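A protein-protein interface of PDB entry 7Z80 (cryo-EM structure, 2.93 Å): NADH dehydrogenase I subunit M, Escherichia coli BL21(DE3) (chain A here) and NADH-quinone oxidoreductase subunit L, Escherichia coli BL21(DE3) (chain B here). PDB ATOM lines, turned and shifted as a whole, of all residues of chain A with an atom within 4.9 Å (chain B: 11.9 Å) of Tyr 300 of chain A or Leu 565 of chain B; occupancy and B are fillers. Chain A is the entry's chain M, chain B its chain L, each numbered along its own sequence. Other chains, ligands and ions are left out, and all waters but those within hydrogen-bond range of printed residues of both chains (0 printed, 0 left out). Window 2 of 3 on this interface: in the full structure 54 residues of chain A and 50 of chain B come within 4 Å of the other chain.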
ATOM      1  N   VAL A 238      25.892 -28.829 -26.261  1.00  0.00           N
ATOM      2  CA  VAL A 238      26.003 -27.457 -25.752  1.00  0.00           C
ATOM      3  C   VAL A 238      25.691 -26.470 -26.873  1.00  0.00           C
ATOM      4  O   VAL A 238      26.004 -26.749 -28.050  1.00  0.00           O
ATOM      5  CB  VAL A 238      27.406 -27.211 -25.167  1.00  0.00           C
ATOM      6  CG1 VAL A 238      27.590 -28.012 -23.892  1.00  0.00           C
ATOM      7  CG2 VAL A 238      28.483 -27.569 -26.176  1.00  0.00           C
ATOM      8  N   PRO A 239      25.052 -25.321 -26.593  1.00  0.00           N
ATOM      9  CA  PRO A 239      24.606 -24.827 -25.286  1.00  0.00           C
ATOM     10  C   PRO A 239      23.223 -25.327 -24.879  1.00  0.00           C
ATOM     11  O   PRO A 239      22.670 -24.862 -23.883  1.00  0.00           O
ATOM     12  CB  PRO A 239      24.584 -23.315 -25.490  1.00  0.00           C
ATOM     13  CG  PRO A 239      24.203 -23.160 -26.916  1.00  0.00           C
ATOM     14  CD  PRO A 239      24.782 -24.341 -27.660  1.00  0.00           C
ATOM     15  N   HIS A 241      21.942 -27.694 -23.216  1.00  0.00           N
ATOM     16  CA  HIS A 241      22.226 -28.739 -22.244  1.00  0.00           C
ATOM     17  C   HIS A 241      21.814 -28.396 -20.821  1.00  0.00           C
ATOM     18  O   HIS A 241      22.032 -29.220 -19.928  1.00  0.00           O
ATOM     19  CB  HIS A 241      23.723 -29.064 -22.249  1.00  0.00           C
ATOM     20  CG  HIS A 241      24.554 -28.035 -21.551  1.00  0.00           C
ATOM     21  ND1 HIS A 241      24.885 -26.830 -22.131  1.00  0.00           N
ATOM     22  CD2 HIS A 241      25.100 -28.019 -20.313  1.00  0.00           C
ATOM     23  CE1 HIS A 241      25.609 -26.120 -21.285  1.00  0.00           C
ATOM     24  NE2 HIS A 241      25.753 -26.819 -20.173  1.00  0.00           N
ATOM     25  N   VAL A 295      33.335 -31.436 -29.649  1.00  0.00           N
ATOM     26  CA  VAL A 295      34.567 -31.078 -28.938  1.00  0.00           C
ATOM     27  C   VAL A 295      34.266 -30.131 -27.779  1.00  0.00           C
ATOM     28  O   VAL A 295      34.717 -30.338 -26.637  1.00  0.00           O
ATOM     29  CB  VAL A 295      35.580 -30.453 -29.914  1.00  0.00           C
ATOM     30  CG1 VAL A 295      36.712 -29.791 -29.160  1.00  0.00           C
ATOM     31  CG2 VAL A 295      36.128 -31.496 -30.856  1.00  0.00           C
ATOM     32  N   ILE A 296      33.494 -29.076 -28.065  1.00  0.00           N
ATOM     33  CA  ILE A 296      33.119 -28.107 -27.041  1.00  0.00           C
ATOM     34  C   ILE A 296      32.289 -28.777 -25.956  1.00  0.00           C
ATOM     35  O   ILE A 296      32.453 -28.487 -24.769  1.00  0.00           O
ATOM     36  CB  ILE A 296      32.382 -26.913 -27.678  1.00  0.00           C
ATOM     37  CG1 ILE A 296      33.312 -26.155 -28.621  1.00  0.00           C
ATOM     38  CG2 ILE A 296      31.860 -25.955 -26.623  1.00  0.00           C
ATOM     39  CD1 ILE A 296      32.606 -25.109 -29.448  1.00  0.00           C
ATOM     40  N   GLY A 297      31.420 -29.716 -26.340  1.00  0.00           N
ATOM     41  CA  GLY A 297      30.629 -30.434 -25.356  1.00  0.00           C
ATOM     42  C   GLY A 297      31.465 -31.301 -24.437  1.00  0.00           C
ATOM     43  O   GLY A 297      31.236 -31.324 -23.227  1.00  0.00           O
ATOM     44  N   ILE A 298      32.462 -32.000 -24.993  1.00  0.00           N
ATOM     45  CA  ILE A 298      33.349 -32.838 -24.184  1.00  0.00           C
ATOM     46  C   ILE A 298      34.101 -31.992 -23.167  1.00  0.00           C
ATOM     47  O   ILE A 298      34.083 -32.273 -21.959  1.00  0.00           O
ATOM     48  CB  ILE A 298      34.331 -33.609 -25.085  1.00  0.00           C
ATOM     49  CG1 ILE A 298      33.619 -34.707 -25.862  1.00  0.00           C
ATOM     50  CG2 ILE A 298      35.463 -34.206 -24.265  1.00  0.00           C
ATOM     51  CD1 ILE A 298      34.471 -35.276 -26.954  1.00  0.00           C
ATOM     52  N   PHE A 299      34.743 -30.917 -23.636  1.00  0.00           N
ATOM     53  CA  PHE A 299      35.572 -30.131 -22.726  1.00  0.00           C
ATOM     54  C   PHE A 299      34.728 -29.322 -21.751  1.00  0.00           C
ATOM     55  O   PHE A 299      35.090 -29.189 -20.576  1.00  0.00           O
ATOM     56  CB  PHE A 299      36.516 -29.237 -23.518  1.00  0.00           C
ATOM     57  CG  PHE A 299      37.765 -29.933 -23.922  1.00  0.00           C
ATOM     58  CD1 PHE A 299      38.892 -29.878 -23.124  1.00  0.00           C
ATOM     59  CD2 PHE A 299      37.794 -30.697 -25.069  1.00  0.00           C
ATOM     60  CE1 PHE A 299      40.043 -30.542 -23.489  1.00  0.00           C
ATOM     61  CE2 PHE A 299      38.930 -31.362 -25.431  1.00  0.00           C
ATOM     62  CZ  PHE A 299      40.061 -31.286 -24.646  1.00  0.00           C
ATOM     63  N   TYR A 300      33.589 -28.803 -22.210  1.00  0.00           N
ATOM     64  CA  TYR A 300      32.682 -28.081 -21.334  1.00  0.00           C
ATOM     65  C   TYR A 300      32.117 -28.991 -20.255  1.00  0.00           C
ATOM     66  O   TYR A 300      32.076 -28.609 -19.085  1.00  0.00           O
ATOM     67  CB  TYR A 300      31.560 -27.459 -22.163  1.00  0.00           C
ATOM     68  CG  TYR A 300      30.775 -26.389 -21.448  1.00  0.00           C
ATOM     69  CD1 TYR A 300      31.244 -25.085 -21.371  1.00  0.00           C
ATOM     70  CD2 TYR A 300      29.559 -26.686 -20.848  1.00  0.00           C
ATOM     71  CE1 TYR A 300      30.521 -24.106 -20.716  1.00  0.00           C
ATOM     72  CE2 TYR A 300      28.836 -25.719 -20.194  1.00  0.00           C
ATOM     73  CZ  TYR A 300      29.317 -24.433 -20.131  1.00  0.00           C
ATOM     74  OH  TYR A 300      28.584 -23.476 -19.476  1.00  0.00           O
ATOM     75  N   GLY A 301      31.702 -30.207 -20.623  1.00  0.00           N
ATOM     76  CA  GLY A 301      31.179 -31.134 -19.635  1.00  0.00           C
ATOM     77  C   GLY A 301      32.229 -31.576 -18.639  1.00  0.00           C
ATOM     78  O   GLY A 301      31.931 -31.752 -17.456  1.00  0.00           O
ATOM     79  N   ALA A 302      33.474 -31.744 -19.096  1.00  0.00           N
ATOM     80  CA  ALA A 302      34.560 -32.041 -18.165  1.00  0.00           C
ATOM     81  C   ALA A 302      34.798 -30.887 -17.196  1.00  0.00           C
ATOM     82  O   ALA A 302      34.986 -31.108 -15.992  1.00  0.00           O
ATOM     83  CB  ALA A 302      35.836 -32.367 -18.938  1.00  0.00           C
ATOM     84  N   TRP A 303      34.783 -29.648 -17.700  1.00  0.00           N
ATOM     85  CA  TRP A 303      35.035 -28.492 -16.845  1.00  0.00           C
ATOM     86  C   TRP A 303      33.903 -28.254 -15.852  1.00  0.00           C
ATOM     87  O   TRP A 303      34.158 -27.812 -14.727  1.00  0.00           O
ATOM     88  CB  TRP A 303      35.276 -27.247 -17.699  1.00  0.00           C
ATOM     89  CG  TRP A 303      36.729 -27.007 -17.988  1.00  0.00           C
ATOM     90  CD1 TRP A 303      37.758 -27.062 -17.098  1.00  0.00           C
ATOM     91  CD2 TRP A 303      37.315 -26.692 -19.258  1.00  0.00           C
ATOM     92  NE1 TRP A 303      38.946 -26.791 -17.729  1.00  0.00           N
ATOM     93  CE2 TRP A 303      38.703 -26.563 -19.057  1.00  0.00           C
ATOM     94  CE3 TRP A 303      36.800 -26.500 -20.544  1.00  0.00           C
ATOM     95  CZ2 TRP A 303      39.582 -26.253 -20.092  1.00  0.00           C
ATOM     96  CZ3 TRP A 303      37.675 -26.194 -21.570  1.00  0.00           C
ATOM     97  CH2 TRP A 303      39.051 -26.073 -21.338  1.00  0.00           C
ATOM     98  N   MET A 304      32.653 -28.513 -16.246  1.00  0.00           N
ATOM     99  CA  MET A 304      31.568 -28.557 -15.268  1.00  0.00           C
ATOM    100  C   MET A 304      31.788 -29.658 -14.242  1.00  0.00           C
ATOM    101  O   MET A 304      31.801 -29.394 -13.037  1.00  0.00           O
ATOM    102  CB  MET A 304      30.209 -28.749 -15.951  1.00  0.00           C
ATOM    103  CG  MET A 304      29.828 -27.849 -17.117  1.00  0.00           C
ATOM    104  SD  MET A 304      30.367 -26.147 -16.982  1.00  0.00           S
ATOM    105  CE  MET A 304      29.402 -25.699 -15.540  1.00  0.00           C
ATOM    106  N   PHE B 553      43.698 -24.548 -15.467  1.00  0.00           N
ATOM    107  CA  PHE B 553      42.584 -25.489 -15.383  1.00  0.00           C
ATOM    108  C   PHE B 553      41.664 -25.146 -14.217  1.00  0.00           C
ATOM    109  O   PHE B 553      40.438 -25.094 -14.375  1.00  0.00           O
ATOM    110  CB  PHE B 553      43.112 -26.918 -15.258  1.00  0.00           C
ATOM    111  CG  PHE B 553      42.045 -27.940 -14.984  1.00  0.00           C
ATOM    112  CD1 PHE B 553      41.221 -28.385 -16.000  1.00  0.00           C
ATOM    113  CD2 PHE B 553      41.870 -28.460 -13.712  1.00  0.00           C
ATOM    114  CE1 PHE B 553      40.239 -29.323 -15.755  1.00  0.00           C
ATOM    115  CE2 PHE B 553      40.890 -29.397 -13.463  1.00  0.00           C
ATOM    116  CZ  PHE B 553      40.074 -29.830 -14.487  1.00  0.00           C
ATOM    117  N   GLY B 555      41.483 -22.184 -12.802  1.00  0.00           N
ATOM    118  CA  GLY B 555      40.889 -20.890 -13.099  1.00  0.00           C
ATOM    119  C   GLY B 555      39.706 -20.983 -14.045  1.00  0.00           C
ATOM    120  O   GLY B 555      38.672 -20.347 -13.822  1.00  0.00           O
ATOM    121  N   ILE B 556      39.832 -21.794 -15.096  1.00  0.00           N
ATOM    122  CA  ILE B 556      38.740 -21.973 -16.046  1.00  0.00           C
ATOM    123  C   ILE B 556      37.580 -22.717 -15.395  1.00  0.00           C
ATOM    124  O   ILE B 556      36.412 -22.397 -15.642  1.00  0.00           O
ATOM    125  CB  ILE B 556      39.259 -22.682 -17.314  1.00  0.00           C
ATOM    126  CG1 ILE B 556      40.134 -21.726 -18.124  1.00  0.00           C
ATOM    127  CG2 ILE B 556      38.121 -23.178 -18.191  1.00  0.00           C
ATOM    128  CD1 ILE B 556      40.757 -22.353 -19.346  1.00  0.00           C
ATOM    129  N   ALA B 557      37.875 -23.690 -14.525  1.00  0.00           N
ATOM    130  CA  ALA B 557      36.810 -24.393 -13.812  1.00  0.00           C
ATOM    131  C   ALA B 557      36.045 -23.457 -12.883  1.00  0.00           C
ATOM    132  O   ALA B 557      34.809 -23.490 -12.840  1.00  0.00           O
ATOM    133  CB  ALA B 557      37.391 -25.568 -13.027  1.00  0.00           C
ATOM    134  N   TRP B 558      36.761 -22.599 -12.151  1.00  0.00           N
ATOM    135  CA  TRP B 558      36.099 -21.646 -11.264  1.00  0.00           C
ATOM    136  C   TRP B 558      35.317 -20.602 -12.054  1.00  0.00           C
ATOM    137  O   TRP B 558      34.250 -20.156 -11.617  1.00  0.00           O
ATOM    138  CB  TRP B 558      37.129 -20.972 -10.357  1.00  0.00           C
ATOM    139  CG  TRP B 558      36.577 -19.827  -9.569  1.00  0.00           C
ATOM    140  CD1 TRP B 558      35.887 -19.897  -8.395  1.00  0.00           C
ATOM    141  CD2 TRP B 558      36.663 -18.436  -9.901  1.00  0.00           C
ATOM    142  NE1 TRP B 558      35.539 -18.637  -7.975  1.00  0.00           N
ATOM    143  CE2 TRP B 558      36.004 -17.722  -8.882  1.00  0.00           C
ATOM    144  CE3 TRP B 558      37.233 -17.725 -10.962  1.00  0.00           C
ATOM    145  CZ2 TRP B 558      35.900 -16.333  -8.891  1.00  0.00           C
ATOM    146  CZ3 TRP B 558      37.128 -16.346 -10.969  1.00  0.00           C
ATOM    147  CH2 TRP B 558      36.467 -15.665  -9.940  1.00  0.00           C
ATOM    148  N   LEU B 559      35.833 -20.198 -13.216  1.00  0.00           N
ATOM    149  CA  LEU B 559      35.116 -19.245 -14.055  1.00  0.00           C
ATOM    150  C   LEU B 559      33.871 -19.866 -14.678  1.00  0.00           C
ATOM    151  O   LEU B 559      32.859 -19.176 -14.854  1.00  0.00           O
ATOM    152  CB  LEU B 559      36.052 -18.711 -15.139  1.00  0.00           C
ATOM    153  CG  LEU B 559      35.589 -17.532 -15.992  1.00  0.00           C
ATOM    154  CD1 LEU B 559      36.696 -16.502 -16.094  1.00  0.00           C
ATOM    155  CD2 LEU B 559      35.181 -18.008 -17.376  1.00  0.00           C
ATOM    156  N   LEU B 560      33.919 -21.153 -15.011  1.00  0.00           N
ATOM    157  CA  LEU B 560      32.827 -21.816 -15.706  1.00  0.00           C
ATOM    158  C   LEU B 560      31.821 -22.471 -14.775  1.00  0.00           C
ATOM    159  O   LEU B 560      30.758 -22.873 -15.248  1.00  0.00           O
ATOM    160  CB  LEU B 560      33.376 -22.875 -16.669  1.00  0.00           C
ATOM    161  CG  LEU B 560      34.041 -22.395 -17.957  1.00  0.00           C
ATOM    162  CD1 LEU B 560      34.293 -23.572 -18.876  1.00  0.00           C
ATOM    163  CD2 LEU B 560      33.189 -21.349 -18.647  1.00  0.00           C
ATOM    164  N   LYS B 561      32.104 -22.552 -13.468  1.00  0.00           N
ATOM    165  CA  LYS B 561      31.240 -23.288 -12.543  1.00  0.00           C
ATOM    166  C   LYS B 561      29.832 -22.712 -12.430  1.00  0.00           C
ATOM    167  O   LYS B 561      28.940 -23.390 -11.912  1.00  0.00           O
ATOM    168  CB  LYS B 561      31.880 -23.332 -11.154  1.00  0.00           C
ATOM    169  CG  LYS B 561      31.784 -22.026 -10.383  1.00  0.00           C
ATOM    170  CD  LYS B 561      31.719 -22.266  -8.886  1.00  0.00           C
ATOM    171  CE  LYS B 561      31.176 -21.049  -8.154  1.00  0.00           C
ATOM    172  NZ  LYS B 561      29.847 -21.313  -7.535  1.00  0.00           N
ATOM    173  N   ARG B 562      29.609 -21.486 -12.898  1.00  0.00           N
ATOM    174  CA  ARG B 562      28.281 -20.890 -12.924  1.00  0.00           C
ATOM    175  C   ARG B 562      27.463 -21.308 -14.140  1.00  0.00           C
ATOM    176  O   ARG B 562      26.305 -20.891 -14.247  1.00  0.00           O
ATOM    177  CB  ARG B 562      28.399 -19.365 -12.893  1.00  0.00           C
ATOM    178  CG  ARG B 562      29.164 -18.800 -14.077  1.00  0.00           C
ATOM    179  CD  ARG B 562      30.091 -17.672 -13.666  1.00  0.00           C
ATOM    180  NE  ARG B 562      30.855 -17.165 -14.799  1.00  0.00           N
ATOM    181  CZ  ARG B 562      30.441 -16.203 -15.613  1.00  0.00           C
ATOM    182  NH1 ARG B 562      29.270 -15.613 -15.446  1.00  0.00           N
ATOM    183  NH2 ARG B 562      31.222 -15.825 -16.622  1.00  0.00           N
ATOM    184  N   ASP B 563      28.043 -22.108 -15.052  1.00  0.00           N
ATOM    185  CA  ASP B 563      27.440 -22.571 -16.303  1.00  0.00           C
ATOM    186  C   ASP B 563      27.003 -21.396 -17.173  1.00  0.00           C
ATOM    187  O   ASP B 563      25.802 -21.112 -17.257  1.00  0.00           O
ATOM    188  CB  ASP B 563      26.257 -23.506 -16.032  1.00  0.00           C
ATOM    189  CG  ASP B 563      26.068 -24.542 -17.124  1.00  0.00           C
ATOM    190  OD1 ASP B 563      26.440 -24.265 -18.282  1.00  0.00           O
ATOM    191  OD2 ASP B 563      25.543 -25.634 -16.824  1.00  0.00           O
ATOM    192  N   PRO B 564      27.942 -20.672 -17.796  1.00  0.00           N
ATOM    193  CA  PRO B 564      27.557 -19.492 -18.596  1.00  0.00           C
ATOM    194  C   PRO B 564      26.659 -19.797 -19.786  1.00  0.00           C
ATOM    195  O   PRO B 564      25.843 -18.943 -20.157  1.00  0.00           O
ATOM    196  CB  PRO B 564      28.911 -18.925 -19.051  1.00  0.00           C
ATOM    197  CG  PRO B 564      29.905 -19.486 -18.098  1.00  0.00           C
ATOM    198  CD  PRO B 564      29.403 -20.848 -17.760  1.00  0.00           C
ATOM    199  N   LEU B 565      26.783 -20.976 -20.401  1.00  0.00           N
ATOM    200  CA  LEU B 565      25.910 -21.316 -21.522  1.00  0.00           C
ATOM    201  C   LEU B 565      24.468 -21.515 -21.071  1.00  0.00           C
ATOM    202  O   LEU B 565      23.536 -21.188 -21.817  1.00  0.00           O
ATOM    203  CB  LEU B 565      26.421 -22.568 -22.232  1.00  0.00           C
ATOM    204  CG  LEU B 565      27.815 -22.492 -22.858  1.00  0.00           C
ATOM    205  CD1 LEU B 565      28.042 -23.673 -23.783  1.00  0.00           C
ATOM    206  CD2 LEU B 565      28.014 -21.181 -23.602  1.00  0.00           C
ATOM    207  N   ASN B 566      24.272 -22.036 -19.857  1.00  0.00           N
ATOM    208  CA  ASN B 566      22.926 -22.175 -19.309  1.00  0.00           C
ATOM    209  C   ASN B 566      22.265 -20.815 -19.118  1.00  0.00           C
ATOM    210  O   ASN B 566      21.084 -20.643 -19.430  1.00  0.00           O
ATOM    211  CB  ASN B 566      22.979 -22.941 -17.988  1.00  0.00           C
ATOM    212  CG  ASN B 566      21.605 -23.275 -17.453  1.00  0.00           C
ATOM    213  OD1 ASN B 566      20.645 -23.410 -18.210  1.00  0.00           O
ATOM    214  ND2 ASN B 566      21.502 -23.412 -16.136  1.00  0.00           N
ATOM    215  N   SER B 567      23.017 -19.827 -18.627  1.00  0.00           N
ATOM    216  CA  SER B 567      22.467 -18.482 -18.488  1.00  0.00           C
ATOM    217  C   SER B 567      22.262 -17.814 -19.842  1.00  0.00           C
ATOM    218  O   SER B 567      21.303 -17.049 -20.020  1.00  0.00           O
ATOM    219  CB  SER B 567      23.382 -17.634 -17.607  1.00  0.00           C
ATOM    220  OG  SER B 567      23.678 -18.307 -16.395  1.00  0.00           O
ATOM    221  N   MET B 568      23.141 -18.102 -20.807  1.00  0.00           N
ATOM    222  CA  MET B 568      22.971 -17.581 -22.160  1.00  0.00           C
ATOM    223  C   MET B 568      21.683 -18.099 -22.790  1.00  0.00           C
ATOM    224  O   MET B 568      20.969 -17.353 -23.471  1.00  0.00           O
ATOM    225  CB  MET B 568      24.185 -17.956 -23.012  1.00  0.00           C
ATOM    226  CG  MET B 568      24.016 -17.747 -24.506  1.00  0.00           C
ATOM    227  SD  MET B 568      25.230 -18.673 -25.464  1.00  0.00           S
ATOM    228  CE  MET B 568      24.206 -19.306 -26.789  1.00  0.00           C
ATOM    229  N   MET B 569      21.358 -19.368 -22.553  1.00  0.00           N
ATOM    230  CA  MET B 569      20.107 -19.925 -23.046  1.00  0.00           C
ATOM    231  C   MET B 569      18.911 -19.617 -22.150  1.00  0.00           C
ATOM    232  O   MET B 569      17.772 -19.827 -22.578  1.00  0.00           O
ATOM    233  CB  MET B 569      20.244 -21.438 -23.223  1.00  0.00           C
ATOM    234  CG  MET B 569      21.149 -21.843 -24.371  1.00  0.00           C
ATOM    235  SD  MET B 569      20.398 -21.598 -25.994  1.00  0.00           S
ATOM    236  CE  MET B 569      18.700 -22.075 -25.680  1.00  0.00           C
ATOM    237  N   ASN B 570      19.136 -19.155 -20.921  1.00  0.00           N
ATOM    238  CA  ASN B 570      18.061 -18.675 -20.061  1.00  0.00           C
ATOM    239  C   ASN B 570      17.757 -17.198 -20.267  1.00  0.00           C
ATOM    240  O   ASN B 570      16.796 -16.693 -19.678  1.00  0.00           O
ATOM    241  CB  ASN B 570      18.412 -18.916 -18.590  1.00  0.00           C
ATOM    242  CG  ASN B 570      18.120 -20.333 -18.144  1.00  0.00           C
ATOM    243  OD1 ASN B 570      17.911 -21.224 -18.966  1.00  0.00           O
ATOM    244  ND2 ASN B 570      18.108 -20.548 -16.834  1.00  0.00           N
ATOM    245  N   ILE B 571      18.593 -16.501 -21.044  1.00  0.00           N
ATOM    246  CA  ILE B 571      18.295 -15.114 -21.427  1.00  0.00           C
ATOM    247  C   ILE B 571      16.910 -14.919 -22.058  1.00  0.00           C
ATOM    248  O   ILE B 571      16.192 -14.004 -21.626  1.00  0.00           O
ATOM    249  CB  ILE B 571      19.436 -14.558 -22.305  1.00  0.00           C
ATOM    250  CG1 ILE B 571      20.586 -14.066 -21.427  1.00  0.00           C
ATOM    251  CG2 ILE B 571      18.951 -13.436 -23.215  1.00  0.00           C
ATOM    252  CD1 ILE B 571      21.911 -13.994 -22.146  1.00  0.00           C
ATOM    253  N   PRO B 572      16.469 -15.713 -23.054  1.00  0.00           N
ATOM    254  CA  PRO B 572      15.125 -15.467 -23.611  1.00  0.00           C
ATOM    255  C   PRO B 572      13.980 -15.764 -22.654  1.00  0.00           C
ATOM    256  O   PRO B 572      12.896 -15.204 -22.844  1.00  0.00           O
ATOM    257  CB  PRO B 572      15.072 -16.378 -24.849  1.00  0.00           C
ATOM    258  CG  PRO B 572      16.464 -16.808 -25.079  1.00  0.00           C
ATOM    259  CD  PRO B 572      17.074 -16.870 -23.741  1.00  0.00           C
ATOM    260  N   ALA B 573      14.180 -16.591 -21.625  1.00  0.00           N
ATOM    261  CA  ALA B 573      13.165 -16.713 -20.581  1.00  0.00           C
ATOM    262  C   ALA B 573      13.008 -15.403 -19.815  1.00  0.00           C
ATOM    263  O   ALA B 573      11.884 -14.981 -19.512  1.00  0.00           O
ATOM    264  CB  ALA B 573      13.519 -17.854 -19.630  1.00  0.00           C
ATOM    265  N   VAL B 574      14.129 -14.741 -19.514  1.00  0.00           N
ATOM    266  CA  VAL B 574      14.091 -13.436 -18.858  1.00  0.00           C
ATOM    267  C   VAL B 574      13.446 -12.402 -19.771  1.00  0.00           C
ATOM    268  O   VAL B 574      12.674 -11.546 -19.319  1.00  0.00           O
ATOM    269  CB  VAL B 574      15.511 -13.015 -18.435  1.00  0.00           C
ATOM    270  CG1 VAL B 574      15.483 -11.703 -17.670  1.00  0.00           C
ATOM    271  CG2 VAL B 574      16.164 -14.109 -17.606  1.00  0.00           C
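A ring nitrogen (NE2) of His 241 of chain A is in hydrogen-bond range of the side-chain carboxylate (OD1) of Asp 563 of chain B (3.3 Å).
The side-chain hydroxyl of Tyr 300 of chain A lies within hydrogen-bond range of the side-chain carboxylate of Asp 563 of chain B, at 2.6 Å.
OH of Tyr 300 of chain A is in hydrogen-bond range of N of Leu 565 of chain B (3.2 Å).
OH of Tyr 300 of chain A sits close to N of Pro 564 of chain B (3.3 Å).
The side-chain sulfur of Met 304 of chain A sits close to the backbone carbonyl oxygen of Leu 560 of chain B (3.7 Å).
The backbone carbonyl oxygen of Pro 239 of chain A is in hydrogen-bond range of a ring nitrogen (ND1) of His 241 of chain A (3.4 Å).
N of Asn 566 of chain B sits at hydrogen-bond distance from OD1 of Asp 563 of chain B (3.5 Å).
Val 238 of chain A touches Leu 565 of chain B (CB to CD1, 3.9 Å).
Pro 239 of chain A touches Leu 565 of chain B (CB to CB, 3.8 Å).
CG of Pro 239 of chain A touches CE of Met 568 of chain B, at 3.9 Å.
CG of Met 569 of chain B touches O of Pro 239 of chain A, at 3.4 Å.
CE1 of His 241 of chain A touches CB of Leu 565 of chain B, 3.8 Å away.
Phe 553 of chain B touches Trp 303 of chain A.
Trp 303 of chain A touches Ile 556 of chain B (CE2 to CG2, 3.5 Å).
CD1 of Leu 560 of chain B touches CB of Trp 303 of chain A, 3.98 Å away.
Met 304 of chain A touches Asp 563 of chain B (CE to CA, 3.8 Å).
Tyr 300 of chain A touches just these residues of chain B: Asp 563 (2.6 Å), Pro 564 (3.2 Å) and Leu 565 (3.2 Å).
Leu 565 of chain B touches just these residues of chain A: Val 238, Pro 239, His 241 and Tyr 300.
Of chain B, only Leu 565 comes within 4 Å of Val 238 of chain A.
Pro 239 of chain A touches three residues of chain B.
Of chain B, only Asp 563 (3.3 Å) and Leu 565 (3.8 Å) come within 4 Å of His 241 of chain A.
Ile 296 of chain A touches none of the printed residues of chain B.
No residue of chain B comes within 4 Å of Gly 297 of chain A.
No residue of chain B comes within 4 Å of Phe 299 of chain A.
No residue of chain B comes within 4 Å of Gly 301 of chain A.
No residue of chain B comes within 4 Å of Ala 302 of chain A.
Met 304 of chain A touches just these residues of chain B: Leu 560 and Asp 563.
Printed residues of chain B within 4 Å of Trp 303 of chain A: Phe 553, Ile 556 and Leu 560.
Printed residues of chain A within 4 Å of Leu 560 of chain B: Trp 303 (3.98 Å) and Met 304 (3.1 Å).
Of the printed residues of chain A, Met 569 of chain B touches Pro 239.
Lys 561 of chain B touches none of the printed residues of chain A.
The nearest residue of chain B that does not touch Tyr 300 of chain A is Leu 560 of chain B (4.2 Å).
The nearest printed residue of chain A that does not touch Leu 565 of chain B is Ile 296 of chain A (5.3 Å).
Of the 13 printed residues of chain A, 6 touch a printed residue of chain B.
Printed residues of chain B that touch a printed residue of chain A: Phe 553, Ile 556, Leu 560, Asp 563, Pro 564, Leu 565, Met 568 and Met 569.
Hydrophobic or aromatic side chains of chain B that line the printed part of chain A: Phe 553, Ile 556, Leu 560, Pro 564, Leu 565, Met 568 and Met 569.
Among the printed residues, no Asp or Glu carboxylate lies within 4 Å of a Lys or Arg side-chain nitrogen of the other chain.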
